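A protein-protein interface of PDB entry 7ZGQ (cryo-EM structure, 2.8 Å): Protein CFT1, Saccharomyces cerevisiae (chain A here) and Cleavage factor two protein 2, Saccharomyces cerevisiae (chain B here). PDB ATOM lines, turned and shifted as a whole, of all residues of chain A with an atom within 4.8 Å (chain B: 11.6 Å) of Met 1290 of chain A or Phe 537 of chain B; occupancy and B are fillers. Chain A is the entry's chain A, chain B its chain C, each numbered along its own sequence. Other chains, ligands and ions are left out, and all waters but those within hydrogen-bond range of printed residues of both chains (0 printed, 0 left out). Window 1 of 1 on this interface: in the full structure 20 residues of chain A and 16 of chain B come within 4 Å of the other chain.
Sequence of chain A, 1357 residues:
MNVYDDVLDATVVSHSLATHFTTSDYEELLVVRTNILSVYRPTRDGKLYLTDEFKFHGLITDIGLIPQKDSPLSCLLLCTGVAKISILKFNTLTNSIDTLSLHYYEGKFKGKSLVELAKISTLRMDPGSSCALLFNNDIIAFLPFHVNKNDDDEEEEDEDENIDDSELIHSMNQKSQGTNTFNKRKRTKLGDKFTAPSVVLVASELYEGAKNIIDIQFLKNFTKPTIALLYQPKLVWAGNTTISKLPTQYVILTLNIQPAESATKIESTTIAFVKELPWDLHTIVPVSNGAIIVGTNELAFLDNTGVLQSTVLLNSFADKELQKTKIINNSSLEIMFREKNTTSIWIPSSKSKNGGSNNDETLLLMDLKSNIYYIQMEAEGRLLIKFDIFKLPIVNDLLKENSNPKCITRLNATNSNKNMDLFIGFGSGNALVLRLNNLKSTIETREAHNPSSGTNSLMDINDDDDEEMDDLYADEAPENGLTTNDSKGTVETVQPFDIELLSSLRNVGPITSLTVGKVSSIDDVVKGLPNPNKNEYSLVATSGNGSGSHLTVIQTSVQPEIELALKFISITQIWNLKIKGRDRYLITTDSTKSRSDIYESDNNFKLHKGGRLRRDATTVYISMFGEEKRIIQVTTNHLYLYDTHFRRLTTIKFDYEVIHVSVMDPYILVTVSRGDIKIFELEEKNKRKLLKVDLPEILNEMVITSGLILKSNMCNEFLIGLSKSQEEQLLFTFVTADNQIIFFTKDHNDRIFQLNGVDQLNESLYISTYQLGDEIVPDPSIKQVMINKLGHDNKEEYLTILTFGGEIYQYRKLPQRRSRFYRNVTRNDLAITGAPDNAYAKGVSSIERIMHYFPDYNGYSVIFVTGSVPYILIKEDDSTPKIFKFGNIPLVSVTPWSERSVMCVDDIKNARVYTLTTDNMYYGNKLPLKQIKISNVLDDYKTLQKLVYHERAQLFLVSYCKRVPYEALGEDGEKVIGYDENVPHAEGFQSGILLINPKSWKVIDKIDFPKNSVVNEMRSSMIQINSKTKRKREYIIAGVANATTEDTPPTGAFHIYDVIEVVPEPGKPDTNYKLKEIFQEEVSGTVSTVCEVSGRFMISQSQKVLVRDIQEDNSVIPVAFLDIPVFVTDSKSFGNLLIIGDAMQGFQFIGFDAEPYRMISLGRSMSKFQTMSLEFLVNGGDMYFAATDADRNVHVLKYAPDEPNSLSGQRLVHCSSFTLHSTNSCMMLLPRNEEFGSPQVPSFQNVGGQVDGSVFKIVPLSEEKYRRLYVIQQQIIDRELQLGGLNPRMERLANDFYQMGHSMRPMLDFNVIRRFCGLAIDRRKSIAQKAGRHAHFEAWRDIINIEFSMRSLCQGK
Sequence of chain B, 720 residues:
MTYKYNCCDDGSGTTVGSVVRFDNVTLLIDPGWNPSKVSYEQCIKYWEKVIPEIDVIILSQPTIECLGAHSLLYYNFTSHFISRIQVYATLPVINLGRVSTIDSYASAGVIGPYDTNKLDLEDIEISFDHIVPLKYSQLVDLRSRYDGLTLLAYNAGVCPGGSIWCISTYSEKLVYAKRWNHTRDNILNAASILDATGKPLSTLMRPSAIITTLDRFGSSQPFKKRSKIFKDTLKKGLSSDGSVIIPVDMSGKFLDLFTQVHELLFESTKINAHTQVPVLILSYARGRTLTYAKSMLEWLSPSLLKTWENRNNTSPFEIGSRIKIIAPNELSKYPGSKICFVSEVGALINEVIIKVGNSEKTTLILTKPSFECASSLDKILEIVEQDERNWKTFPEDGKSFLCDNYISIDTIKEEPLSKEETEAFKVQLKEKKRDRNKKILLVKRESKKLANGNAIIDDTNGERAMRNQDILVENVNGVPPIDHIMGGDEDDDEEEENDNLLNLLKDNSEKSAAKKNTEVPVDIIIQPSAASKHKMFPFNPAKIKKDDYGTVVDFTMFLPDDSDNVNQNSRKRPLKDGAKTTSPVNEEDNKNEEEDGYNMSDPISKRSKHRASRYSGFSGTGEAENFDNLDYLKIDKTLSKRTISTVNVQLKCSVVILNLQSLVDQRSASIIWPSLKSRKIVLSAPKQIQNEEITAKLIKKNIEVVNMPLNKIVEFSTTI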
ATOM      1  N   LYS A  84       5.174 -21.624 -27.152  1.00  0.00           N
ATOM      2  CA  LYS A  84       4.682 -22.964 -27.436  1.00  0.00           C
ATOM      3  C   LYS A  84       4.877 -23.281 -28.909  1.00  0.00           C
ATOM      4  O   LYS A  84       4.691 -22.416 -29.769  1.00  0.00           O
ATOM      5  CB  LYS A  84       3.203 -23.112 -27.076  1.00  0.00           C
ATOM      6  CG  LYS A  84       2.948 -23.778 -25.744  1.00  0.00           C
ATOM      7  CD  LYS A  84       1.473 -24.074 -25.584  1.00  0.00           C
ATOM      8  CE  LYS A  84       0.639 -22.811 -25.701  1.00  0.00           C
ATOM      9  NZ  LYS A  84      -0.623 -22.888 -24.916  1.00  0.00           N
ATOM     10  N   ILE A  85       5.255 -24.525 -29.189  1.00  0.00           N
ATOM     11  CA  ILE A  85       5.400 -25.018 -30.554  1.00  0.00           C
ATOM     12  C   ILE A  85       4.796 -26.415 -30.615  1.00  0.00           C
ATOM     13  O   ILE A  85       5.165 -27.289 -29.823  1.00  0.00           O
ATOM     14  CB  ILE A  85       6.869 -25.037 -31.010  1.00  0.00           C
ATOM     15  CG1 ILE A  85       7.256 -23.678 -31.597  1.00  0.00           C
ATOM     16  CG2 ILE A  85       7.116 -26.152 -32.006  1.00  0.00           C
ATOM     17  CD1 ILE A  85       8.697 -23.587 -32.033  1.00  0.00           C
ATOM     18  N   SER A  86       3.864 -26.623 -31.542  1.00  0.00           N
ATOM     19  CA  SER A  86       3.238 -27.922 -31.748  1.00  0.00           C
ATOM     20  C   SER A  86       3.285 -28.265 -33.228  1.00  0.00           C
ATOM     21  O   SER A  86       2.878 -27.458 -34.069  1.00  0.00           O
ATOM     22  CB  SER A  86       1.791 -27.929 -31.245  1.00  0.00           C
ATOM     23  OG  SER A  86       0.989 -27.028 -31.984  1.00  0.00           O
ATOM     24  N   LEU A 102       5.301 -32.008 -29.484  1.00  0.00           N
ATOM     25  CA  LEU A 102       5.015 -30.822 -28.692  1.00  0.00           C
ATOM     26  C   LEU A 102       6.308 -30.260 -28.120  1.00  0.00           C
ATOM     27  O   LEU A 102       7.257 -30.998 -27.841  1.00  0.00           O
ATOM     28  CB  LEU A 102       4.036 -31.135 -27.557  1.00  0.00           C
ATOM     29  CG  LEU A 102       2.640 -31.608 -27.966  1.00  0.00           C
ATOM     30  CD1 LEU A 102       1.866 -32.098 -26.754  1.00  0.00           C
ATOM     31  CD2 LEU A 102       1.881 -30.500 -28.671  1.00  0.00           C
ATOM     32  N   HIS A 103       6.344 -28.939 -27.957  1.00  0.00           N
ATOM     33  CA  HIS A 103       7.512 -28.250 -27.419  1.00  0.00           C
ATOM     34  C   HIS A 103       7.037 -27.083 -26.570  1.00  0.00           C
ATOM     35  O   HIS A 103       6.391 -26.165 -27.082  1.00  0.00           O
ATOM     36  CB  HIS A 103       8.435 -27.770 -28.541  1.00  0.00           C
ATOM     37  CG  HIS A 103       8.797 -28.841 -29.522  1.00  0.00           C
ATOM     38  ND1 HIS A 103       9.829 -29.729 -29.307  1.00  0.00           N
ATOM     39  CD2 HIS A 103       8.250 -29.183 -30.712  1.00  0.00           C
ATOM     40  CE1 HIS A 103       9.911 -30.562 -30.329  1.00  0.00           C
ATOM     41  NE2 HIS A 103       8.964 -30.252 -31.195  1.00  0.00           N
ATOM     42  N   TYR A 104       7.359 -27.120 -25.280  1.00  0.00           N
ATOM     43  CA  TYR A 104       6.884 -26.140 -24.306  1.00  0.00           C
ATOM     44  C   TYR A 104       8.086 -25.360 -23.781  1.00  0.00           C
ATOM     45  O   TYR A 104       8.795 -25.824 -22.884  1.00  0.00           O
ATOM     46  CB  TYR A 104       6.131 -26.837 -23.178  1.00  0.00           C
ATOM     47  CG  TYR A 104       5.592 -25.902 -22.125  1.00  0.00           C
ATOM     48  CD1 TYR A 104       4.571 -25.009 -22.420  1.00  0.00           C
ATOM     49  CD2 TYR A 104       6.102 -25.912 -20.834  1.00  0.00           C
ATOM     50  CE1 TYR A 104       4.073 -24.154 -21.460  1.00  0.00           C
ATOM     51  CE2 TYR A 104       5.612 -25.059 -19.868  1.00  0.00           C
ATOM     52  CZ  TYR A 104       4.597 -24.183 -20.185  1.00  0.00           C
ATOM     53  OH  TYR A 104       4.104 -23.330 -19.226  1.00  0.00           O
ATOM     54  N   GLY A1285      -3.134 -30.778 -29.721  1.00  0.00           N
ATOM     55  CA  GLY A1285      -2.501 -31.014 -28.438  1.00  0.00           C
ATOM     56  C   GLY A1285      -2.634 -29.852 -27.484  1.00  0.00           C
ATOM     57  O   GLY A1285      -1.751 -29.637 -26.649  1.00  0.00           O
ATOM     58  N   LEU A1286      -3.725 -29.098 -27.580  1.00  0.00           N
ATOM     59  CA  LEU A1286      -3.942 -27.914 -26.760  1.00  0.00           C
ATOM     60  C   LEU A1286      -4.860 -28.275 -25.600  1.00  0.00           C
ATOM     61  O   LEU A1286      -5.980 -28.748 -25.814  1.00  0.00           O
ATOM     62  CB  LEU A1286      -4.547 -26.781 -27.589  1.00  0.00           C
ATOM     63  CG  LEU A1286      -3.756 -26.306 -28.810  1.00  0.00           C
ATOM     64  CD1 LEU A1286      -4.227 -24.930 -29.249  1.00  0.00           C
ATOM     65  CD2 LEU A1286      -2.265 -26.294 -28.521  1.00  0.00           C
ATOM     66  N   ASN A1287      -4.383 -28.057 -24.382  1.00  0.00           N
ATOM     67  CA  ASN A1287      -5.199 -28.294 -23.202  1.00  0.00           C
ATOM     68  C   ASN A1287      -6.060 -27.067 -22.933  1.00  0.00           C
ATOM     69  O   ASN A1287      -5.514 -25.994 -22.654  1.00  0.00           O
ATOM     70  CB  ASN A1287      -4.320 -28.594 -21.996  1.00  0.00           C
ATOM     71  CG  ASN A1287      -5.110 -29.086 -20.799  1.00  0.00           C
ATOM     72  OD1 ASN A1287      -6.340 -29.075 -20.802  1.00  0.00           O
ATOM     73  ND2 ASN A1287      -4.403 -29.523 -19.766  1.00  0.00           N
ATOM     74  N   PRO A1288      -7.390 -27.173 -23.011  1.00  0.00           N
ATOM     75  CA  PRO A1288      -8.227 -25.993 -22.734  1.00  0.00           C
ATOM     76  C   PRO A1288      -8.019 -25.428 -21.343  1.00  0.00           C
ATOM     77  O   PRO A1288      -8.068 -24.205 -21.160  1.00  0.00           O
ATOM     78  CB  PRO A1288      -9.650 -26.533 -22.931  1.00  0.00           C
ATOM     79  CG  PRO A1288      -9.480 -27.673 -23.877  1.00  0.00           C
ATOM     80  CD  PRO A1288      -8.190 -28.318 -23.470  1.00  0.00           C
ATOM     81  N   ARG A1289      -7.770 -26.291 -20.354  1.00  0.00           N
ATOM     82  CA  ARG A1289      -7.512 -25.807 -19.004  1.00  0.00           C
ATOM     83  C   ARG A1289      -6.284 -24.913 -18.969  1.00  0.00           C
ATOM     84  O   ARG A1289      -6.273 -23.891 -18.279  1.00  0.00           O
ATOM     85  CB  ARG A1289      -7.339 -26.979 -18.038  1.00  0.00           C
ATOM     86  CG  ARG A1289      -8.630 -27.664 -17.645  1.00  0.00           C
ATOM     87  CD  ARG A1289      -8.846 -28.923 -18.456  1.00  0.00           C
ATOM     88  NE  ARG A1289      -7.935 -29.988 -18.052  1.00  0.00           N
ATOM     89  CZ  ARG A1289      -8.285 -31.041 -17.326  1.00  0.00           C
ATOM     90  NH1 ARG A1289      -9.529 -31.208 -16.906  1.00  0.00           N
ATOM     91  NH2 ARG A1289      -7.365 -31.949 -17.015  1.00  0.00           N
ATOM     92  N   MET A1290      -5.237 -25.278 -19.704  1.00  0.00           N
ATOM     93  CA  MET A1290      -4.036 -24.457 -19.710  1.00  0.00           C
ATOM     94  C   MET A1290      -4.122 -23.322 -20.724  1.00  0.00           C
ATOM     95  O   MET A1290      -3.438 -22.307 -20.566  1.00  0.00           O
ATOM     96  CB  MET A1290      -2.814 -25.347 -19.951  1.00  0.00           C
ATOM     97  CG  MET A1290      -1.566 -24.667 -20.452  1.00  0.00           C
ATOM     98  SD  MET A1290      -0.488 -25.826 -21.296  1.00  0.00           S
ATOM     99  CE  MET A1290       0.360 -24.723 -22.405  1.00  0.00           C
ATOM    100  N   GLU A1291      -4.976 -23.451 -21.742  1.00  0.00           N
ATOM    101  CA  GLU A1291      -5.217 -22.324 -22.633  1.00  0.00           C
ATOM    102  C   GLU A1291      -5.994 -21.213 -21.936  1.00  0.00           C
ATOM    103  O   GLU A1291      -5.829 -20.037 -22.281  1.00  0.00           O
ATOM    104  CB  GLU A1291      -5.966 -22.781 -23.885  1.00  0.00           C
ATOM    105  CG  GLU A1291      -5.191 -23.736 -24.779  1.00  0.00           C
ATOM    106  CD  GLU A1291      -3.780 -23.264 -25.067  1.00  0.00           C
ATOM    107  OE1 GLU A1291      -3.601 -22.075 -25.405  1.00  0.00           O
ATOM    108  OE2 GLU A1291      -2.847 -24.086 -24.959  1.00  0.00           O
ATOM    109  N   ARG A1292      -6.837 -21.556 -20.962  1.00  0.00           N
ATOM    110  CA  ARG A1292      -7.689 -20.574 -20.298  1.00  0.00           C
ATOM    111  C   ARG A1292      -7.188 -20.169 -18.916  1.00  0.00           C
ATOM    112  O   ARG A1292      -7.005 -18.979 -18.649  1.00  0.00           O
ATOM    113  CB  ARG A1292      -9.120 -21.113 -20.190  1.00  0.00           C
ATOM    114  CG  ARG A1292      -9.752 -21.474 -21.523  1.00  0.00           C
ATOM    115  CD  ARG A1292      -9.776 -20.286 -22.468  1.00  0.00           C
ATOM    116  NE  ARG A1292     -10.767 -20.456 -23.523  1.00  0.00           N
ATOM    117  CZ  ARG A1292     -11.130 -19.505 -24.372  1.00  0.00           C
ATOM    118  NH1 ARG A1292     -10.600 -18.294 -24.320  1.00  0.00           N
ATOM    119  NH2 ARG A1292     -12.047 -19.774 -25.296  1.00  0.00           N
ATOM    120  N   LEU A1293      -6.966 -21.133 -18.025  1.00  0.00           N
ATOM    121  CA  LEU A1293      -6.671 -20.842 -16.628  1.00  0.00           C
ATOM    122  C   LEU A1293      -5.202 -20.549 -16.355  1.00  0.00           C
ATOM    123  O   LEU A1293      -4.881 -20.079 -15.259  1.00  0.00           O
ATOM    124  CB  LEU A1293      -7.120 -22.011 -15.750  1.00  0.00           C
ATOM    125  CG  LEU A1293      -8.608 -22.348 -15.809  1.00  0.00           C
ATOM    126  CD1 LEU A1293      -8.818 -23.851 -15.780  1.00  0.00           C
ATOM    127  CD2 LEU A1293      -9.339 -21.678 -14.662  1.00  0.00           C
ATOM    128  N   ALA A1294      -4.303 -20.808 -17.306  1.00  0.00           N
ATOM    129  CA  ALA A1294      -2.874 -20.596 -17.078  1.00  0.00           C
ATOM    130  C   ALA A1294      -2.545 -19.133 -17.356  1.00  0.00           C
ATOM    131  O   ALA A1294      -1.965 -18.768 -18.381  1.00  0.00           O
ATOM    132  CB  ALA A1294      -2.040 -21.539 -17.934  1.00  0.00           C
ATOM    133  N   ILE B 524      10.227 -31.437 -26.899  1.00  0.00           N
ATOM    134  CA  ILE B 524      10.188 -31.873 -25.510  1.00  0.00           C
ATOM    135  C   ILE B 524       9.382 -33.160 -25.387  1.00  0.00           C
ATOM    136  O   ILE B 524       9.786 -34.095 -24.696  1.00  0.00           O
ATOM    137  CB  ILE B 524       9.615 -30.769 -24.600  1.00  0.00           C
ATOM    138  CG1 ILE B 524      10.651 -29.663 -24.399  1.00  0.00           C
ATOM    139  CG2 ILE B 524       9.193 -31.337 -23.252  1.00  0.00           C
ATOM    140  CD1 ILE B 524      10.259 -28.637 -23.365  1.00  0.00           C
ATOM    141  N   ILE B 525       8.244 -33.213 -26.072  1.00  0.00           N
ATOM    142  CA  ILE B 525       7.349 -34.365 -26.023  1.00  0.00           C
ATOM    143  C   ILE B 525       7.268 -34.967 -27.418  1.00  0.00           C
ATOM    144  O   ILE B 525       6.940 -34.268 -28.386  1.00  0.00           O
ATOM    145  CB  ILE B 525       5.952 -33.985 -25.508  1.00  0.00           C
ATOM    146  CG1 ILE B 525       6.056 -33.279 -24.154  1.00  0.00           C
ATOM    147  CG2 ILE B 525       5.072 -35.223 -25.401  1.00  0.00           C
ATOM    148  CD1 ILE B 525       4.734 -32.765 -23.630  1.00  0.00           C
ATOM    149  N   ILE B 526       7.501 -36.276 -27.537  1.00  0.00           N
ATOM    150  CA  ILE B 526       7.279 -36.935 -28.860  1.00  0.00           C
ATOM    151  C   ILE B 526       5.881 -37.559 -28.801  1.00  0.00           C
ATOM    152  O   ILE B 526       5.580 -38.204 -27.781  1.00  0.00           O
ATOM    153  CB  ILE B 526       8.377 -37.962 -29.181  1.00  0.00           C
ATOM    154  CG1 ILE B 526       9.757 -37.304 -29.237  1.00  0.00           C
ATOM    155  CG2 ILE B 526       8.054 -38.706 -30.468  1.00  0.00           C
ATOM    156  CD1 ILE B 526       9.829 -36.124 -30.178  1.00  0.00           C
ATOM    157  N   GLN B 527       5.059 -37.367 -29.837  1.00  0.00           N
ATOM    158  CA  GLN B 527       3.648 -37.842 -29.781  1.00  0.00           C
ATOM    159  C   GLN B 527       3.496 -39.227 -30.415  1.00  0.00           C
ATOM    160  O   GLN B 527       3.476 -39.305 -31.658  1.00  0.00           O
ATOM    161  CB  GLN B 527       2.732 -36.841 -30.486  1.00  0.00           C
ATOM    162  CG  GLN B 527       2.477 -35.577 -29.678  1.00  0.00           C
ATOM    163  CD  GLN B 527       1.644 -35.862 -28.453  1.00  0.00           C
ATOM    164  OE1 GLN B 527       1.500 -35.023 -27.568  1.00  0.00           O
ATOM    165  NE2 GLN B 527       1.089 -37.061 -28.391  1.00  0.00           N
ATOM    166  N   PRO B 528       3.375 -40.316 -29.623  1.00  0.00           N
ATOM    167  CA  PRO B 528       3.122 -41.650 -30.162  1.00  0.00           C
ATOM    168  C   PRO B 528       1.619 -41.954 -30.090  1.00  0.00           C
ATOM    169  O   PRO B 528       0.932 -41.307 -29.320  1.00  0.00           O
ATOM    170  CB  PRO B 528       3.892 -42.521 -29.168  1.00  0.00           C
ATOM    171  CG  PRO B 528       3.688 -41.820 -27.840  1.00  0.00           C
ATOM    172  CD  PRO B 528       3.528 -40.347 -28.168  1.00  0.00           C
ATOM    173  N   ALA B 531      -2.058 -43.363 -26.186  1.00  0.00           N
ATOM    174  CA  ALA B 531      -2.909 -42.839 -25.131  1.00  0.00           C
ATOM    175  C   ALA B 531      -4.005 -41.959 -25.732  1.00  0.00           C
ATOM    176  O   ALA B 531      -4.185 -41.895 -26.949  1.00  0.00           O
ATOM    177  CB  ALA B 531      -2.059 -42.078 -24.110  1.00  0.00           C
ATOM    178  N   SER B 532      -4.775 -41.297 -24.869  1.00  0.00           N
ATOM    179  CA  SER B 532      -5.782 -40.339 -25.311  1.00  0.00           C
ATOM    180  C   SER B 532      -5.508 -38.938 -24.782  1.00  0.00           C
ATOM    181  O   SER B 532      -5.420 -37.991 -25.571  1.00  0.00           O
ATOM    182  CB  SER B 532      -7.177 -40.811 -24.883  1.00  0.00           C
ATOM    183  OG  SER B 532      -8.009 -39.706 -24.580  1.00  0.00           O
ATOM    184  N   LYS B 533      -5.358 -38.779 -23.470  1.00  0.00           N
ATOM    185  CA  LYS B 533      -5.150 -37.476 -22.854  1.00  0.00           C
ATOM    186  C   LYS B 533      -3.680 -37.114 -22.709  1.00  0.00           C
ATOM    187  O   LYS B 533      -3.371 -36.035 -22.194  1.00  0.00           O
ATOM    188  CB  LYS B 533      -5.828 -37.431 -21.480  1.00  0.00           C
ATOM    189  CG  LYS B 533      -5.105 -38.221 -20.404  1.00  0.00           C
ATOM    190  CD  LYS B 533      -5.968 -38.381 -19.163  1.00  0.00           C
ATOM    191  CE  LYS B 533      -6.899 -39.577 -19.289  1.00  0.00           C
ATOM    192  NZ  LYS B 533      -7.592 -39.883 -18.006  1.00  0.00           N
ATOM    193  N   HIS B 534      -2.769 -37.983 -23.139  1.00  0.00           N
ATOM    194  CA  HIS B 534      -1.343 -37.696 -23.087  1.00  0.00           C
ATOM    195  C   HIS B 534      -0.813 -37.090 -24.380  1.00  0.00           C
ATOM    196  O   HIS B 534       0.385 -36.802 -24.465  1.00  0.00           O
ATOM    197  CB  HIS B 534      -0.563 -38.968 -22.748  1.00  0.00           C
ATOM    198  CG  HIS B 534      -0.894 -39.530 -21.400  1.00  0.00           C
ATOM    199  ND1 HIS B 534      -1.083 -38.735 -20.290  1.00  0.00           N
ATOM    200  CD2 HIS B 534      -1.072 -40.806 -20.985  1.00  0.00           C
ATOM    201  CE1 HIS B 534      -1.364 -39.498 -19.249  1.00  0.00           C
ATOM    202  NE2 HIS B 534      -1.362 -40.758 -19.642  1.00  0.00           N
ATOM    203  N   LYS B 535      -1.667 -36.889 -25.382  1.00  0.00           N
ATOM    204  CA  LYS B 535      -1.305 -36.135 -26.573  1.00  0.00           C
ATOM    205  C   LYS B 535      -1.528 -34.638 -26.405  1.00  0.00           C
ATOM    206  O   LYS B 535      -1.631 -33.918 -27.404  1.00  0.00           O
ATOM    207  CB  LYS B 535      -2.078 -36.641 -27.792  1.00  0.00           C
ATOM    208  CG  LYS B 535      -2.019 -38.141 -28.015  1.00  0.00           C
ATOM    209  CD  LYS B 535      -3.345 -38.673 -28.521  1.00  0.00           C
ATOM    210  CE  LYS B 535      -3.181 -40.051 -29.134  1.00  0.00           C
ATOM    211  NZ  LYS B 535      -2.378 -40.017 -30.384  1.00  0.00           N
ATOM    212  N   MET B 536      -1.601 -34.161 -25.170  1.00  0.00           N
ATOM    213  CA  MET B 536      -1.898 -32.775 -24.850  1.00  0.00           C
ATOM    214  C   MET B 536      -0.694 -32.130 -24.170  1.00  0.00           C
ATOM    215  O   MET B 536       0.303 -32.785 -23.861  1.00  0.00           O
ATOM    216  CB  MET B 536      -3.130 -32.685 -23.948  1.00  0.00           C
ATOM    217  CG  MET B 536      -4.440 -32.475 -24.678  1.00  0.00           C
ATOM    218  SD  MET B 536      -5.861 -32.460 -23.565  1.00  0.00           S
ATOM    219  CE  MET B 536      -5.064 -32.359 -21.967  1.00  0.00           C
ATOM    220  N   PHE B 537      -0.801 -30.829 -23.943  1.00  0.00           N
ATOM    221  CA  PHE B 537       0.133 -30.146 -23.060  1.00  0.00           C
ATOM    222  C   PHE B 537      -0.261 -30.407 -21.611  1.00  0.00           C
ATOM    223  O   PHE B 537      -1.407 -30.143 -21.232  1.00  0.00           O
ATOM    224  CB  PHE B 537       0.147 -28.646 -23.330  1.00  0.00           C
ATOM    225  CG  PHE B 537       0.956 -28.249 -24.529  1.00  0.00           C
ATOM    226  CD1 PHE B 537       2.331 -28.400 -24.531  1.00  0.00           C
ATOM    227  CD2 PHE B 537       0.347 -27.708 -25.645  1.00  0.00           C
ATOM    228  CE1 PHE B 537       3.079 -28.031 -25.631  1.00  0.00           C
ATOM    229  CE2 PHE B 537       1.090 -27.338 -26.749  1.00  0.00           C
ATOM    230  CZ  PHE B 537       2.458 -27.498 -26.740  1.00  0.00           C
ATOM    231  N   PRO B 538       0.639 -30.939 -20.785  1.00  0.00           N
ATOM    232  CA  PRO B 538       0.294 -31.182 -19.376  1.00  0.00           C
ATOM    233  C   PRO B 538      -0.014 -29.876 -18.658  1.00  0.00           C
ATOM    234  O   PRO B 538       0.612 -28.847 -18.917  1.00  0.00           O
ATOM    235  CB  PRO B 538       1.550 -31.857 -18.811  1.00  0.00           C
ATOM    236  CG  PRO B 538       2.326 -32.317 -20.012  1.00  0.00           C
ATOM    237  CD  PRO B 538       2.025 -31.327 -21.087  1.00  0.00           C
ATOM    238  N   PHE B 539      -0.990 -29.924 -17.753  1.00  0.00           N
ATOM    239  CA  PHE B 539      -1.370 -28.769 -16.942  1.00  0.00           C
ATOM    240  C   PHE B 539      -1.821 -29.259 -15.571  1.00  0.00           C
ATOM    241  O   PHE B 539      -2.955 -29.717 -15.407  1.00  0.00           O
ATOM    242  CB  PHE B 539      -2.465 -27.953 -17.617  1.00  0.00           C
ATOM    243  CG  PHE B 539      -2.950 -26.794 -16.792  1.00  0.00           C
ATOM    244  CD1 PHE B 539      -2.179 -25.651 -16.657  1.00  0.00           C
ATOM    245  CD2 PHE B 539      -4.180 -26.844 -16.160  1.00  0.00           C
ATOM    246  CE1 PHE B 539      -2.626 -24.583 -15.908  1.00  0.00           C
ATOM    247  CE2 PHE B 539      -4.629 -25.780 -15.404  1.00  0.00           C
ATOM    248  CZ  PHE B 539      -3.851 -24.648 -15.278  1.00  0.00           C
ATOM    249  N   ASN B 540      -0.927 -29.157 -14.588  1.00  0.00           N
ATOM    250  CA  ASN B 540      -1.247 -29.493 -13.201  1.00  0.00           C
ATOM    251  C   ASN B 540      -0.362 -28.673 -12.270  1.00  0.00           C
ATOM    252  O   ASN B 540       0.499 -29.210 -11.564  1.00  0.00           O
ATOM    253  CB  ASN B 540      -1.090 -30.994 -12.959  1.00  0.00           C
ATOM    254  CG  ASN B 540       0.319 -31.490 -13.236  1.00  0.00           C
ATOM    255  OD1 ASN B 540       0.943 -31.101 -14.223  1.00  0.00           O
ATOM    256  ND2 ASN B 540       0.824 -32.353 -12.363  1.00  0.00           N
ATOM    257  N   PRO B 541      -0.553 -27.354 -12.239  1.00  0.00           N
ATOM    258  CA  PRO B 541       0.237 -26.528 -11.320  1.00  0.00           C
ATOM    259  C   PRO B 541      -0.118 -26.844  -9.877  1.00  0.00           C
ATOM    260  O   PRO B 541      -1.289 -26.830  -9.491  1.00  0.00           O
ATOM    261  CB  PRO B 541      -0.155 -25.094 -11.701  1.00  0.00           C
ATOM    262  CG  PRO B 541      -0.777 -25.205 -13.054  1.00  0.00           C
ATOM    263  CD  PRO B 541      -1.462 -26.531 -13.054  1.00  0.00           C
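The backbone NH (N) of Ile 524 of chain B lies within hydrogen-bond range of the backbone carbonyl oxygen (O) of Leu 102 of chain A, 3.1 Å away. The backbone carbonyl oxygen of Gly 1285 of chain A sits close to the backbone NH of Phe 537 of chain B (3.1 Å). The backbone carbonyl oxygen of Phe 537 of chain B sits close to the side-chain amide nitrogen of Asn 1287 of chain A (3.4 Å). O of Ile 525 of chain B lies within hydrogen-bond range of N of Leu 102 of chain A (3.0 Å). N of Ile 524 of chain B is in hydrogen-bond range of ND1 of His 103 of chain A.
The backbone NH of Arg 1289 of chain A lies within hydrogen-bond range of the side-chain amide oxygen of Asn 1287 of chain A (3.2 Å). The side-chain amide oxygen (OE1) of Gln 527 of chain B sits close to the backbone carbonyl oxygen (O) of Lys 535 of chain B.
Among the printed residues, merely in contact across the chains: Lys 84 of chain A with Phe 537 of chain B (3.5 Å), Leu 102 of chain A with Gln 527 of chain B (3.1 Å), Leu 102 of chain A with Lys 535 of chain B (3.995 Å), Leu 102 of chain A with Met 536 of chain B (3.4 Å), Leu 102 of chain A with Phe 537 of chain B (3.6 Å), Tyr 104 of chain A with Ile 524 of chain B (3.2 Å), Gly 1285 of chain A with Lys 535 of chain B (3.2 Å), Gly 1285 of chain A with Met 536 of chain B (3.6 Å), Leu 1286 of chain A with Phe 537 of chain B (3.9 Å), Asn 1287 of chain A with Met 536 of chain B (3.5 Å), Asn 1287 of chain A with Phe 539 of chain B (3.3 Å), Arg 1289 of chain A with Phe 539 of chain B (3.7 Å), Met 1290 of chain A with Phe 537 of chain B (3.5 Å), Met 1290 of chain A with Pro 538 of chain B (3.9995 Å), Met 1290 of chain A with Phe 539 of chain B (3.4 Å) and Ala 1294 of chain A with Phe 539 of chain B (3.7 Å).
Printed residues of chain B within 4 Å of Tyr 104 of chain A: Ile 524 (3.2 Å). Of chain B, only Lys 535, Met 536 and Phe 537 come within 4 Å of Gly 1285 of chain A. Of chain B, only Phe 537 (3.9 Å) comes within 4 Å of Leu 1286 of chain A. No residue of chain B comes within 4 Å of Glu 1291 of chain A. Of the printed residues of chain A, Phe 539 of chain B touches Asn 1287 (3.3 Å), Arg 1289 (3.7 Å), Met 1290 (3.4 Å) and Ala 1294 (3.7 Å). Printed residues of chain A within 4 Å of Ile 525 of chain B: Leu 102 (3.0 Å).
Hydrophobic or aromatic side chains of chain A within 4 Å of the printed part of chain B: Leu 102, His 103, Leu 1286, Met 1290 and Ala 1294. Hydrophobic or aromatic side chains of chain B within 4 Å of the printed part of chain A: Ile 524, Ile 525, Met 536, Phe 537 and Phe 539. Among the printed residues, 21 pairs touch across the chains.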
